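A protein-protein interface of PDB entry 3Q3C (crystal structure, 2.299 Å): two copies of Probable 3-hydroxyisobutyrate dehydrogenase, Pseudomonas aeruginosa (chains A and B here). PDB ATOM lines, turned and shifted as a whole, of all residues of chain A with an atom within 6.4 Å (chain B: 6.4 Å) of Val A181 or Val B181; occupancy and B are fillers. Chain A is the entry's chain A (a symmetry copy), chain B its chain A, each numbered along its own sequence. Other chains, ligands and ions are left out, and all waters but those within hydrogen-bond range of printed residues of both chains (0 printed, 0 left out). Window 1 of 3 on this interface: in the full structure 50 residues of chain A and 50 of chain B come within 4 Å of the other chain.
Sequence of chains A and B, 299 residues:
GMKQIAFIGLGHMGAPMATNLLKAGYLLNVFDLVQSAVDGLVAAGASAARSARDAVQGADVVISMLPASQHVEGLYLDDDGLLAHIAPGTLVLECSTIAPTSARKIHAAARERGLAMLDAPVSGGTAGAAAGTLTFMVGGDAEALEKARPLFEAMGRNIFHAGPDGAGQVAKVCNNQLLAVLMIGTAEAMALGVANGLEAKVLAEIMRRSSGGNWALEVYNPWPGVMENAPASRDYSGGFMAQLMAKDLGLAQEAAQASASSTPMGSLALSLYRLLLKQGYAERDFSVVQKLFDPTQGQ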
ATOM      1  N   ASN A 176      11.090  -3.888  28.181  1.00  0.00           N
ATOM      2  CA  ASN A 176      10.296  -2.875  27.499  1.00  0.00           C
ATOM      3  C   ASN A 176      11.153  -1.754  26.958  1.00  0.00           C
ATOM      4  O   ASN A 176      10.807  -1.132  25.942  1.00  0.00           O
ATOM      5  CB  ASN A 176       9.170  -2.331  28.391  1.00  0.00           C
ATOM      6  CG  ASN A 176       7.897  -3.170  28.309  1.00  0.00           C
ATOM      7  OD1 ASN A 176       7.953  -4.381  28.062  1.00  0.00           O
ATOM      8  ND2 ASN A 176       6.736  -2.528  28.521  1.00  0.00           N
ATOM      9  N   GLN A 177      12.282  -1.509  27.612  1.00  0.00           N
ATOM     10  CA  GLN A 177      13.249  -0.539  27.091  1.00  0.00           C
ATOM     11  C   GLN A 177      13.860  -1.014  25.754  1.00  0.00           C
ATOM     12  O   GLN A 177      13.997  -0.244  24.796  1.00  0.00           O
ATOM     13  CB  GLN A 177      14.365  -0.271  28.097  1.00  0.00           C
ATOM     14  CG  GLN A 177      15.143   0.969  27.729  1.00  0.00           C
ATOM     15  CD  GLN A 177      16.314   1.256  28.635  1.00  0.00           C
ATOM     16  OE1 GLN A 177      16.553   2.404  29.006  1.00  0.00           O
ATOM     17  NE2 GLN A 177      17.080   0.230  28.958  1.00  0.00           N
ATOM     18  N   LEU A 178      14.232  -2.289  25.702  1.00  0.00           N
ATOM     19  CA  LEU A 178      14.754  -2.863  24.474  1.00  0.00           C
ATOM     20  C   LEU A 178      13.681  -2.853  23.379  1.00  0.00           C
ATOM     21  O   LEU A 178      13.967  -2.550  22.208  1.00  0.00           O
ATOM     22  CB  LEU A 178      15.220  -4.294  24.733  1.00  0.00           C
ATOM     23  CG  LEU A 178      15.801  -5.079  23.560  1.00  0.00           C
ATOM     24  CD1 LEU A 178      16.718  -4.233  22.714  1.00  0.00           C
ATOM     25  CD2 LEU A 178      16.561  -6.312  24.075  1.00  0.00           C
ATOM     26  N   LEU A 179      12.449  -3.195  23.761  1.00  0.00           N
ATOM     27  CA  LEU A 179      11.320  -3.034  22.853  1.00  0.00           C
ATOM     28  C   LEU A 179      11.277  -1.611  22.249  1.00  0.00           C
ATOM     29  O   LEU A 179      11.116  -1.443  21.038  1.00  0.00           O
ATOM     30  CB  LEU A 179      10.003  -3.355  23.553  1.00  0.00           C
ATOM     31  CG  LEU A 179       8.773  -2.989  22.717  1.00  0.00           C
ATOM     32  CD1 LEU A 179       8.799  -3.753  21.414  1.00  0.00           C
ATOM     33  CD2 LEU A 179       7.498  -3.294  23.491  1.00  0.00           C
ATOM     34  N   ALA A 180      11.422  -0.587  23.082  1.00  0.00           N
ATOM     35  CA  ALA A 180      11.278   0.760  22.575  1.00  0.00           C
ATOM     36  C   ALA A 180      12.362   0.959  21.534  1.00  0.00           C
ATOM     37  O   ALA A 180      12.153   1.553  20.469  1.00  0.00           O
ATOM     38  CB  ALA A 180      11.398   1.793  23.704  1.00  0.00           C
ATOM     39  N   VAL A 181      13.531   0.432  21.846  1.00  0.00           N
ATOM     40  CA  VAL A 181      14.682   0.621  20.993  1.00  0.00           C
ATOM     41  C   VAL A 181      14.483  -0.069  19.640  1.00  0.00           C
ATOM     42  O   VAL A 181      14.720   0.532  18.594  1.00  0.00           O
ATOM     43  CB  VAL A 181      15.942   0.105  21.683  1.00  0.00           C
ATOM     44  CG1 VAL A 181      17.059  -0.065  20.700  1.00  0.00           C
ATOM     45  CG2 VAL A 181      16.329   1.053  22.839  1.00  0.00           C
ATOM     46  N   LEU A 182      14.036  -1.325  19.650  1.00  0.00           N
ATOM     47  CA  LEU A 182      13.920  -2.045  18.391  1.00  0.00           C
ATOM     48  C   LEU A 182      12.755  -1.472  17.577  1.00  0.00           C
ATOM     49  O   LEU A 182      12.800  -1.409  16.333  1.00  0.00           O
ATOM     50  CB  LEU A 182      13.835  -3.561  18.615  1.00  0.00           C
ATOM     51  CG  LEU A 182      12.812  -4.164  19.570  1.00  0.00           C
ATOM     52  CD1 LEU A 182      11.465  -4.185  18.906  1.00  0.00           C
ATOM     53  CD2 LEU A 182      13.233  -5.586  19.928  1.00  0.00           C
ATOM     54  N   MET A 183      11.725  -1.002  18.277  1.00  0.00           N
ATOM     55  CA  MET A 183      10.604  -0.414  17.556  1.00  0.00           C
ATOM     56  C   MET A 183      11.046   0.866  16.854  1.00  0.00           C
ATOM     57  O   MET A 183      10.823   1.034  15.646  1.00  0.00           O
ATOM     58  CB  MET A 183       9.400  -0.170  18.467  1.00  0.00           C
ATOM     59  CG  MET A 183       8.273   0.567  17.793  1.00  0.00           C
ATOM     60  SD  MET A 183       7.344  -0.487  16.423  1.00  0.00           S
ATOM     61  CE  MET A 183       6.476  -1.923  17.441  1.00  0.00           C
ATOM     62  N   ILE A 184      11.695   1.768  17.586  1.00  0.00           N
ATOM     63  CA  ILE A 184      12.230   2.953  16.925  1.00  0.00           C
ATOM     64  C   ILE A 184      13.222   2.566  15.801  1.00  0.00           C
ATOM     65  O   ILE A 184      13.170   3.112  14.688  1.00  0.00           O
ATOM     66  CB  ILE A 184      12.886   3.944  17.876  1.00  0.00           C
ATOM     67  CG1 ILE A 184      11.868   4.431  18.915  1.00  0.00           C
ATOM     68  CG2 ILE A 184      13.403   5.149  17.064  1.00  0.00           C
ATOM     69  CD1 ILE A 184      12.425   5.403  19.913  1.00  0.00           C
ATOM     70  N   GLY A 185      14.106   1.619  16.107  1.00  0.00           N
ATOM     71  CA  GLY A 185      15.084   1.169  15.157  1.00  0.00           C
ATOM     72  C   GLY A 185      14.362   0.616  13.952  1.00  0.00           C
ATOM     73  O   GLY A 185      14.804   0.816  12.819  1.00  0.00           O
ATOM     74  N   THR A 186      13.243  -0.066  14.188  1.00  0.00           N
ATOM     75  CA  THR A 186      12.471  -0.586  13.076  1.00  0.00           C
ATOM     76  C   THR A 186      11.802   0.528  12.265  1.00  0.00           C
ATOM     77  O   THR A 186      11.902   0.553  11.029  1.00  0.00           O
ATOM     78  CB  THR A 186      11.481  -1.695  13.498  1.00  0.00           C
ATOM     79  OG1 THR A 186      12.210  -2.780  14.097  1.00  0.00           O
ATOM     80  CG2 THR A 186      10.763  -2.240  12.256  1.00  0.00           C
ATOM     81  N   GLU A 188      12.764   3.654  11.917  1.00  0.00           N
ATOM     82  CA  GLU A 188      13.719   4.462  11.144  1.00  0.00           C
ATOM     83  C   GLU A 188      14.270   3.691   9.936  1.00  0.00           C
ATOM     84  O   GLU A 188      14.496   4.269   8.859  1.00  0.00           O
ATOM     85  CB  GLU A 188      14.853   5.047  12.006  1.00  0.00           C
ATOM     86  CG  GLU A 188      16.022   4.118  12.265  1.00  0.00           C
ATOM     87  CD  GLU A 188      17.168   4.735  13.091  1.00  0.00           C
ATOM     88  OE1 GLU A 188      16.991   5.799  13.746  1.00  0.00           O
ATOM     89  OE2 GLU A 188      18.261   4.119  13.079  1.00  0.00           O
ATOM     90  N   LEU A 249       9.899   3.663  30.061  1.00  0.00           N
ATOM     91  CA  LEU A 249      11.240   4.169  29.804  1.00  0.00           C
ATOM     92  C   LEU A 249      11.723   4.974  30.990  1.00  0.00           C
ATOM     93  O   LEU A 249      12.914   4.995  31.307  1.00  0.00           O
ATOM     94  CB  LEU A 249      11.252   5.045  28.539  1.00  0.00           C
ATOM     95  CG  LEU A 249      11.105   4.203  27.257  1.00  0.00           C
ATOM     96  CD1 LEU A 249      10.980   5.057  25.992  1.00  0.00           C
ATOM     97  CD2 LEU A 249      12.256   3.202  27.123  1.00  0.00           C
ATOM     98  N   MET A 265      20.773   4.149  24.124  1.00  0.00           N
ATOM     99  CA  MET A 265      19.663   3.901  23.207  1.00  0.00           C
ATOM    100  C   MET A 265      18.327   4.108  23.926  1.00  0.00           C
ATOM    101  O   MET A 265      17.481   4.886  23.482  1.00  0.00           O
ATOM    102  CB  MET A 265      19.759   2.480  22.654  1.00  0.00           C
ATOM    103  CG  MET A 265      21.174   2.104  22.214  1.00  0.00           C
ATOM    104  SD  MET A 265      21.795   3.168  20.680  1.00  0.00           S
ATOM    105  CE  MET A 265      20.347   2.744  19.525  1.00  0.00           C
ATOM    106  N   GLY A 266      18.147   3.418  25.049  1.00  0.00           N
ATOM    107  CA  GLY A 266      16.964   3.634  25.865  1.00  0.00           C
ATOM    108  C   GLY A 266      16.681   5.101  26.189  1.00  0.00           C
ATOM    109  O   GLY A 266      15.568   5.581  25.984  1.00  0.00           O
ATOM    110  N   SER A 267      17.676   5.822  26.689  1.00  0.00           N
ATOM    111  CA  SER A 267      17.514   7.267  26.974  1.00  0.00           C
ATOM    112  C   SER A 267      17.137   8.087  25.724  1.00  0.00           C
ATOM    113  O   SER A 267      16.337   9.022  25.787  1.00  0.00           O
ATOM    114  CB  SER A 267      18.810   7.844  27.553  1.00  0.00           C
ATOM    115  OG  SER A 267      19.254   7.073  28.657  1.00  0.00           O
ATOM    116  N   ALA A 269      15.605   6.823  23.085  1.00  0.00           N
ATOM    117  CA  ALA A 269      14.236   6.388  22.823  1.00  0.00           C
ATOM    118  C   ALA A 269      13.286   7.208  23.677  1.00  0.00           C
ATOM    119  O   ALA A 269      12.266   7.684  23.195  1.00  0.00           O
ATOM    120  CB  ALA A 269      14.066   4.899  23.125  1.00  0.00           C
ATOM    121  N   TYR A 273      10.155   9.524  22.434  1.00  0.00           N
ATOM    122  CA  TYR A 273       8.789   9.412  22.905  1.00  0.00           C
ATOM    123  C   TYR A 273       8.259  10.703  23.532  1.00  0.00           C
ATOM    124  O   TYR A 273       7.077  11.001  23.395  1.00  0.00           O
ATOM    125  CB  TYR A 273       8.622   8.223  23.833  1.00  0.00           C
ATOM    126  CG  TYR A 273       8.379   6.988  23.017  1.00  0.00           C
ATOM    127  CD1 TYR A 273       7.114   6.707  22.548  1.00  0.00           C
ATOM    128  CD2 TYR A 273       9.432   6.142  22.653  1.00  0.00           C
ATOM    129  CE1 TYR A 273       6.876   5.597  21.784  1.00  0.00           C
ATOM    130  CE2 TYR A 273       9.202   5.041  21.883  1.00  0.00           C
ATOM    131  CZ  TYR A 273       7.912   4.776  21.444  1.00  0.00           C
ATOM    132  OH  TYR A 273       7.649   3.696  20.654  1.00  0.00           O
ATOM    133  N   ASN B 176      21.517  -3.908   8.284  1.00  0.00           N
ATOM    134  CA  ASN B 176      22.681  -3.953   9.159  1.00  0.00           C
ATOM    135  C   ASN B 176      22.688  -2.813  10.150  1.00  0.00           C
ATOM    136  O   ASN B 176      23.218  -2.950  11.264  1.00  0.00           O
ATOM    137  CB  ASN B 176      23.994  -4.005   8.365  1.00  0.00           C
ATOM    138  CG  ASN B 176      24.403  -5.430   7.996  1.00  0.00           C
ATOM    139  OD1 ASN B 176      23.549  -6.308   7.827  1.00  0.00           O
ATOM    140  ND2 ASN B 176      25.719  -5.665   7.866  1.00  0.00           N
ATOM    141  N   GLN B 177      22.079  -1.697   9.768  1.00  0.00           N
ATOM    142  CA  GLN B 177      21.907  -0.583  10.704  1.00  0.00           C
ATOM    143  C   GLN B 177      20.970  -0.964  11.871  1.00  0.00           C
ATOM    144  O   GLN B 177      21.240  -0.669  13.041  1.00  0.00           O
ATOM    145  CB  GLN B 177      21.368   0.659   9.999  1.00  0.00           C
ATOM    146  CG  GLN B 177      21.533   1.888  10.858  1.00  0.00           C
ATOM    147  CD  GLN B 177      20.953   3.144  10.260  1.00  0.00           C
ATOM    148  OE1 GLN B 177      21.559   4.212  10.330  1.00  0.00           O
ATOM    149  NE2 GLN B 177      19.755   3.041   9.711  1.00  0.00           N
ATOM    150  N   LEU B 178      19.861  -1.618  11.539  1.00  0.00           N
ATOM    151  CA  LEU B 178      18.940  -2.088  12.558  1.00  0.00           C
ATOM    152  C   LEU B 178      19.615  -3.141  13.445  1.00  0.00           C
ATOM    153  O   LEU B 178      19.444  -3.142  14.677  1.00  0.00           O
ATOM    154  CB  LEU B 178      17.699  -2.684  11.895  1.00  0.00           C
ATOM    155  CG  LEU B 178      16.604  -3.243  12.801  1.00  0.00           C
ATOM    156  CD1 LEU B 178      16.350  -2.355  13.992  1.00  0.00           C
ATOM    157  CD2 LEU B 178      15.304  -3.428  12.003  1.00  0.00           C
ATOM    158  N   LEU B 179      20.372  -4.042  12.815  1.00  0.00           N
ATOM    159  CA  LEU B 179      21.210  -4.963  13.573  1.00  0.00           C
ATOM    160  C   LEU B 179      22.081  -4.216  14.609  1.00  0.00           C
ATOM    161  O   LEU B 179      22.155  -4.612  15.774  1.00  0.00           O
ATOM    162  CB  LEU B 179      22.086  -5.798  12.643  1.00  0.00           C
ATOM    163  CG  LEU B 179      23.142  -6.620  13.387  1.00  0.00           C
ATOM    164  CD1 LEU B 179      22.463  -7.566  14.350  1.00  0.00           C
ATOM    165  CD2 LEU B 179      24.005  -7.391  12.399  1.00  0.00           C
ATOM    166  N   ALA B 180      22.740  -3.140  14.194  1.00  0.00           N
ATOM    167  CA  ALA B 180      23.651  -2.478  15.101  1.00  0.00           C
ATOM    168  C   ALA B 180      22.828  -1.993  16.278  1.00  0.00           C
ATOM    169  O   ALA B 180      23.233  -2.077  17.445  1.00  0.00           O
ATOM    170  CB  ALA B 180      24.371  -1.312  14.410  1.00  0.00           C
ATOM    171  N   VAL B 181      21.647  -1.497  15.960  1.00  0.00           N
ATOM    172  CA  VAL B 181      20.792  -0.911  16.969  1.00  0.00           C
ATOM    173  C   VAL B 181      20.324  -1.969  17.973  1.00  0.00           C
ATOM    174  O   VAL B 181      20.398  -1.754  19.181  1.00  0.00           O
ATOM    175  CB  VAL B 181      19.598  -0.222  16.313  1.00  0.00           C
ATOM    176  CG1 VAL B 181      18.520   0.051  17.316  1.00  0.00           C
ATOM    177  CG2 VAL B 181      20.066   1.067  15.602  1.00  0.00           C
ATOM    178  N   LEU B 182      19.852  -3.115  17.484  1.00  0.00           N
ATOM    179  CA  LEU B 182      19.315  -4.108  18.402  1.00  0.00           C
ATOM    180  C   LEU B 182      20.458  -4.739  19.205  1.00  0.00           C
ATOM    181  O   LEU B 182      20.305  -5.084  20.392  1.00  0.00           O
ATOM    182  CB  LEU B 182      18.430  -5.129  17.673  1.00  0.00           C
ATOM    183  CG  LEU B 182      18.936  -5.881  16.448  1.00  0.00           C
ATOM    184  CD1 LEU B 182      19.852  -6.987  16.887  1.00  0.00           C
ATOM    185  CD2 LEU B 182      17.748  -6.466  15.690  1.00  0.00           C
ATOM    186  N   MET B 183      21.627  -4.844  18.578  1.00  0.00           N
ATOM    187  CA  MET B 183      22.758  -5.406  19.303  1.00  0.00           C
ATOM    188  C   MET B 183      23.159  -4.478  20.446  1.00  0.00           C
ATOM    189  O   MET B 183      23.281  -4.911  21.599  1.00  0.00           O
ATOM    190  CB  MET B 183      23.940  -5.707  18.382  1.00  0.00           C
ATOM    191  CG  MET B 183      25.178  -6.153  19.112  1.00  0.00           C
ATOM    192  SD  MET B 183      25.023  -7.937  19.917  1.00  0.00           S
ATOM    193  CE  MET B 183      24.883  -9.140  18.373  1.00  0.00           C
ATOM    194  N   ILE B 184      23.346  -3.193  20.149  1.00  0.00           N
ATOM    195  CA  ILE B 184      23.621  -2.257  21.232  1.00  0.00           C
ATOM    196  C   ILE B 184      22.480  -2.261  22.278  1.00  0.00           C
ATOM    197  O   ILE B 184      22.728  -2.294  23.494  1.00  0.00           O
ATOM    198  CB  ILE B 184      23.887  -0.834  20.763  1.00  0.00           C
ATOM    199  CG1 ILE B 184      25.102  -0.806  19.826  1.00  0.00           C
ATOM    200  CG2 ILE B 184      24.170   0.055  21.991  1.00  0.00           C
ATOM    201  CD1 ILE B 184      25.437   0.555  19.292  1.00  0.00           C
ATOM    202  N   GLY B 185      21.242  -2.238  21.788  1.00  0.00           N
ATOM    203  CA  GLY B 185      20.093  -2.237  22.649  1.00  0.00           C
ATOM    204  C   GLY B 185      20.127  -3.487  23.495  1.00  0.00           C
ATOM    205  O   GLY B 185      19.776  -3.446  24.676  1.00  0.00           O
ATOM    206  N   THR B 186      20.560  -4.597  22.903  1.00  0.00           N
ATOM    207  CA  THR B 186      20.665  -5.825  23.665  1.00  0.00           C
ATOM    208  C   THR B 186      21.783  -5.764  24.710  1.00  0.00           C
ATOM    209  O   THR B 186      21.565  -6.097  25.885  1.00  0.00           O
ATOM    210  CB  THR B 186      20.751  -7.083  22.772  1.00  0.00           C
ATOM    211  OG1 THR B 186      19.578  -7.158  21.943  1.00  0.00           O
ATOM    212  CG2 THR B 186      20.781  -8.338  23.655  1.00  0.00           C
ATOM    213  N   GLU B 188      23.028  -3.114  26.209  1.00  0.00           N
ATOM    214  CA  GLU B 188      22.729  -2.204  27.325  1.00  0.00           C
ATOM    215  C   GLU B 188      21.661  -2.784  28.264  1.00  0.00           C
ATOM    216  O   GLU B 188      21.726  -2.603  29.491  1.00  0.00           O
ATOM    217  CB  GLU B 188      22.363  -0.781  26.863  1.00  0.00           C
ATOM    218  CG  GLU B 188      20.916  -0.578  26.459  1.00  0.00           C
ATOM    219  CD  GLU B 188      20.555   0.861  26.042  1.00  0.00           C
ATOM    220  OE1 GLU B 188      21.458   1.697  25.765  1.00  0.00           O
ATOM    221  OE2 GLU B 188      19.333   1.138  25.987  1.00  0.00           O
ATOM    222  N   LEU B 249      27.522   1.142   8.915  1.00  0.00           N
ATOM    223  CA  LEU B 249      26.804   2.268   9.497  1.00  0.00           C
ATOM    224  C   LEU B 249      27.111   3.530   8.722  1.00  0.00           C
ATOM    225  O   LEU B 249      26.268   4.419   8.587  1.00  0.00           O
ATOM    226  CB  LEU B 249      27.197   2.452  10.973  1.00  0.00           C
ATOM    227  CG  LEU B 249      26.601   1.348  11.868  1.00  0.00           C
ATOM    228  CD1 LEU B 249      27.083   1.429  13.319  1.00  0.00           C
ATOM    229  CD2 LEU B 249      25.071   1.358  11.804  1.00  0.00           C
ATOM    230  N   MET B 265      18.876   6.489  16.013  1.00  0.00           N
ATOM    231  CA  MET B 265      19.435   5.295  16.644  1.00  0.00           C
ATOM    232  C   MET B 265      20.668   4.818  15.870  1.00  0.00           C
ATOM    233  O   MET B 265      21.750   4.658  16.438  1.00  0.00           O
ATOM    234  CB  MET B 265      18.376   4.196  16.695  1.00  0.00           C
ATOM    235  CG  MET B 265      17.011   4.701  17.160  1.00  0.00           C
ATOM    236  SD  MET B 265      17.031   5.317  19.029  1.00  0.00           S
ATOM    237  CE  MET B 265      17.702   3.704  19.778  1.00  0.00           C
ATOM    238  N   GLY B 266      20.503   4.606  14.568  1.00  0.00           N
ATOM    239  CA  GLY B 266      21.639   4.265  13.727  1.00  0.00           C
ATOM    240  C   GLY B 266      22.840   5.200  13.881  1.00  0.00           C
ATOM    241  O   GLY B 266      23.961   4.744  14.091  1.00  0.00           O
ATOM    242  N   SER B 267      22.618   6.504  13.785  1.00  0.00           N
ATOM    243  CA  SER B 267      23.708   7.489  13.983  1.00  0.00           C
ATOM    244  C   SER B 267      24.360   7.388  15.376  1.00  0.00           C
ATOM    245  O   SER B 267      25.574   7.537  15.529  1.00  0.00           O
ATOM    246  CB  SER B 267      23.177   8.913  13.803  1.00  0.00           C
ATOM    247  OG  SER B 267      22.487   9.042  12.571  1.00  0.00           O
ATOM    248  N   ALA B 269      24.362   4.646  17.218  1.00  0.00           N
ATOM    249  CA  ALA B 269      25.080   3.378  17.141  1.00  0.00           C
ATOM    250  C   ALA B 269      26.434   3.615  16.498  1.00  0.00           C
ATOM    251  O   ALA B 269      27.448   3.123  16.976  1.00  0.00           O
ATOM    252  CB  ALA B 269      24.287   2.346  16.337  1.00  0.00           C
ATOM    253  N   TYR B 273      30.127   2.770  18.034  1.00  0.00           N
ATOM    254  CA  TYR B 273      31.145   1.971  17.381  1.00  0.00           C
ATOM    255  C   TYR B 273      32.457   2.728  17.162  1.00  0.00           C
ATOM    256  O   TYR B 273      33.522   2.124  17.238  1.00  0.00           O
ATOM    257  CB  TYR B 273      30.624   1.359  16.094  1.00  0.00           C
ATOM    258  CG  TYR B 273      29.906   0.080  16.409  1.00  0.00           C
ATOM    259  CD1 TYR B 273      30.619  -1.086  16.591  1.00  0.00           C
ATOM    260  CD2 TYR B 273      28.521   0.055  16.601  1.00  0.00           C
ATOM    261  CE1 TYR B 273      29.985  -2.258  16.900  1.00  0.00           C
ATOM    262  CE2 TYR B 273      27.885  -1.107  16.919  1.00  0.00           C
ATOM    263  CZ  TYR B 273      28.631  -2.269  17.073  1.00  0.00           C
ATOM    264  OH  TYR B 273      28.032  -3.445  17.414  1.00  0.00           O
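Hydrophobic or aromatic side chains of chain A that line the printed part of chain B: Leu A178, Val A181, Ile A184 and Met A265.
Of the 18 printed residues of chain B, 9 touch a printed residue of chain A.
Hydrophobic or aromatic side chains of chain B within 4 Å of the printed part of chain A: Leu B178, Val B181, Ile B184 and Met B265.
Among the printed residues, no Asp or Glu carboxylate lies within 4 Å of a Lys or Arg side-chain nitrogen of the other chain.
The backbone carbonyl oxygen (O) of Leu B182 lies within hydrogen-bond range of the side-chain hydroxyl (OG1) of Thr B186, 2.7 Å away.
The backbone carbonyl oxygen (O) of Leu A182 lies within hydrogen-bond range of the side-chain hydroxyl (OG1) of Thr A186 (2.7 Å).
Val A181 touches two residues of chain B.
Val B181 touches two residues of chain A.
Of the printed residues of chain B, Ile A184 touches Met B265.
Of the printed residues of chain A, Ile B184 touches Met A265.
The nearest residue of chain B that does not touch Val A181 is Gly B185 (4.2 Å).
The nearest residue of chain A that does not touch Val B181 is Gly A185 (4.2 Å).
The nearest printed residue of chain A that does not touch Gly B266 is Met A265 (5.3 Å).
Among the printed residues, pairs that only touch across the chains: Gln A177 with Glu B188 (3.8 Å), Leu A178 with Gly B185 (3.6 Å), Leu A178 with Thr B186 (3.8 Å), Val A181 with Val B181 (3.7 Å), Val A181 with Met B265 (3.9 Å), Ile A184 with Met B265 (3.6 Å), Gly A185 with Leu B178 (3.6 Å), Thr A186 with Leu B178 (3.8 Å), Glu A188 with Gln B177 (3.8 Å), Met A265 with Val B181 (3.9 Å), Met A265 with Ile B184 (3.6 Å) and Met A265 with Met B265 (2.8 Å).
The side-chain carboxylate (OE1) of Glu B188 sits at hydrogen-bond distance from the backbone NH (N) of Met A265 (3.0 Å).
The backbone NH of Gly A266 sits at hydrogen-bond distance from the side-chain carboxylate of Glu B188, 2.7 Å away.
N of Met B265 is in hydrogen-bond range of OE1 of Glu A188, 3.0 Å away.
The backbone NH of Gly B266 lies within hydrogen-bond range of the side-chain carboxylate of Glu A188, at 2.7 Å.
Leu A178 touches Gly B185, and with the chains exchanged Gly A185 touches Leu B178.
Leu A178 touches Thr B186, and with the chains exchanged Thr A186 touches Leu B178.
Val B181 touches its own counterpart, Val A181.
Glu A188 touches Met B265, and with the chains exchanged Met A265 touches Glu B188.
Positions printed for both chains: 176, 177, 178, 179, 180, 181, 182, 183, 184, 185, 186, 188, 249, 265, 266, 267, 269 and 273.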
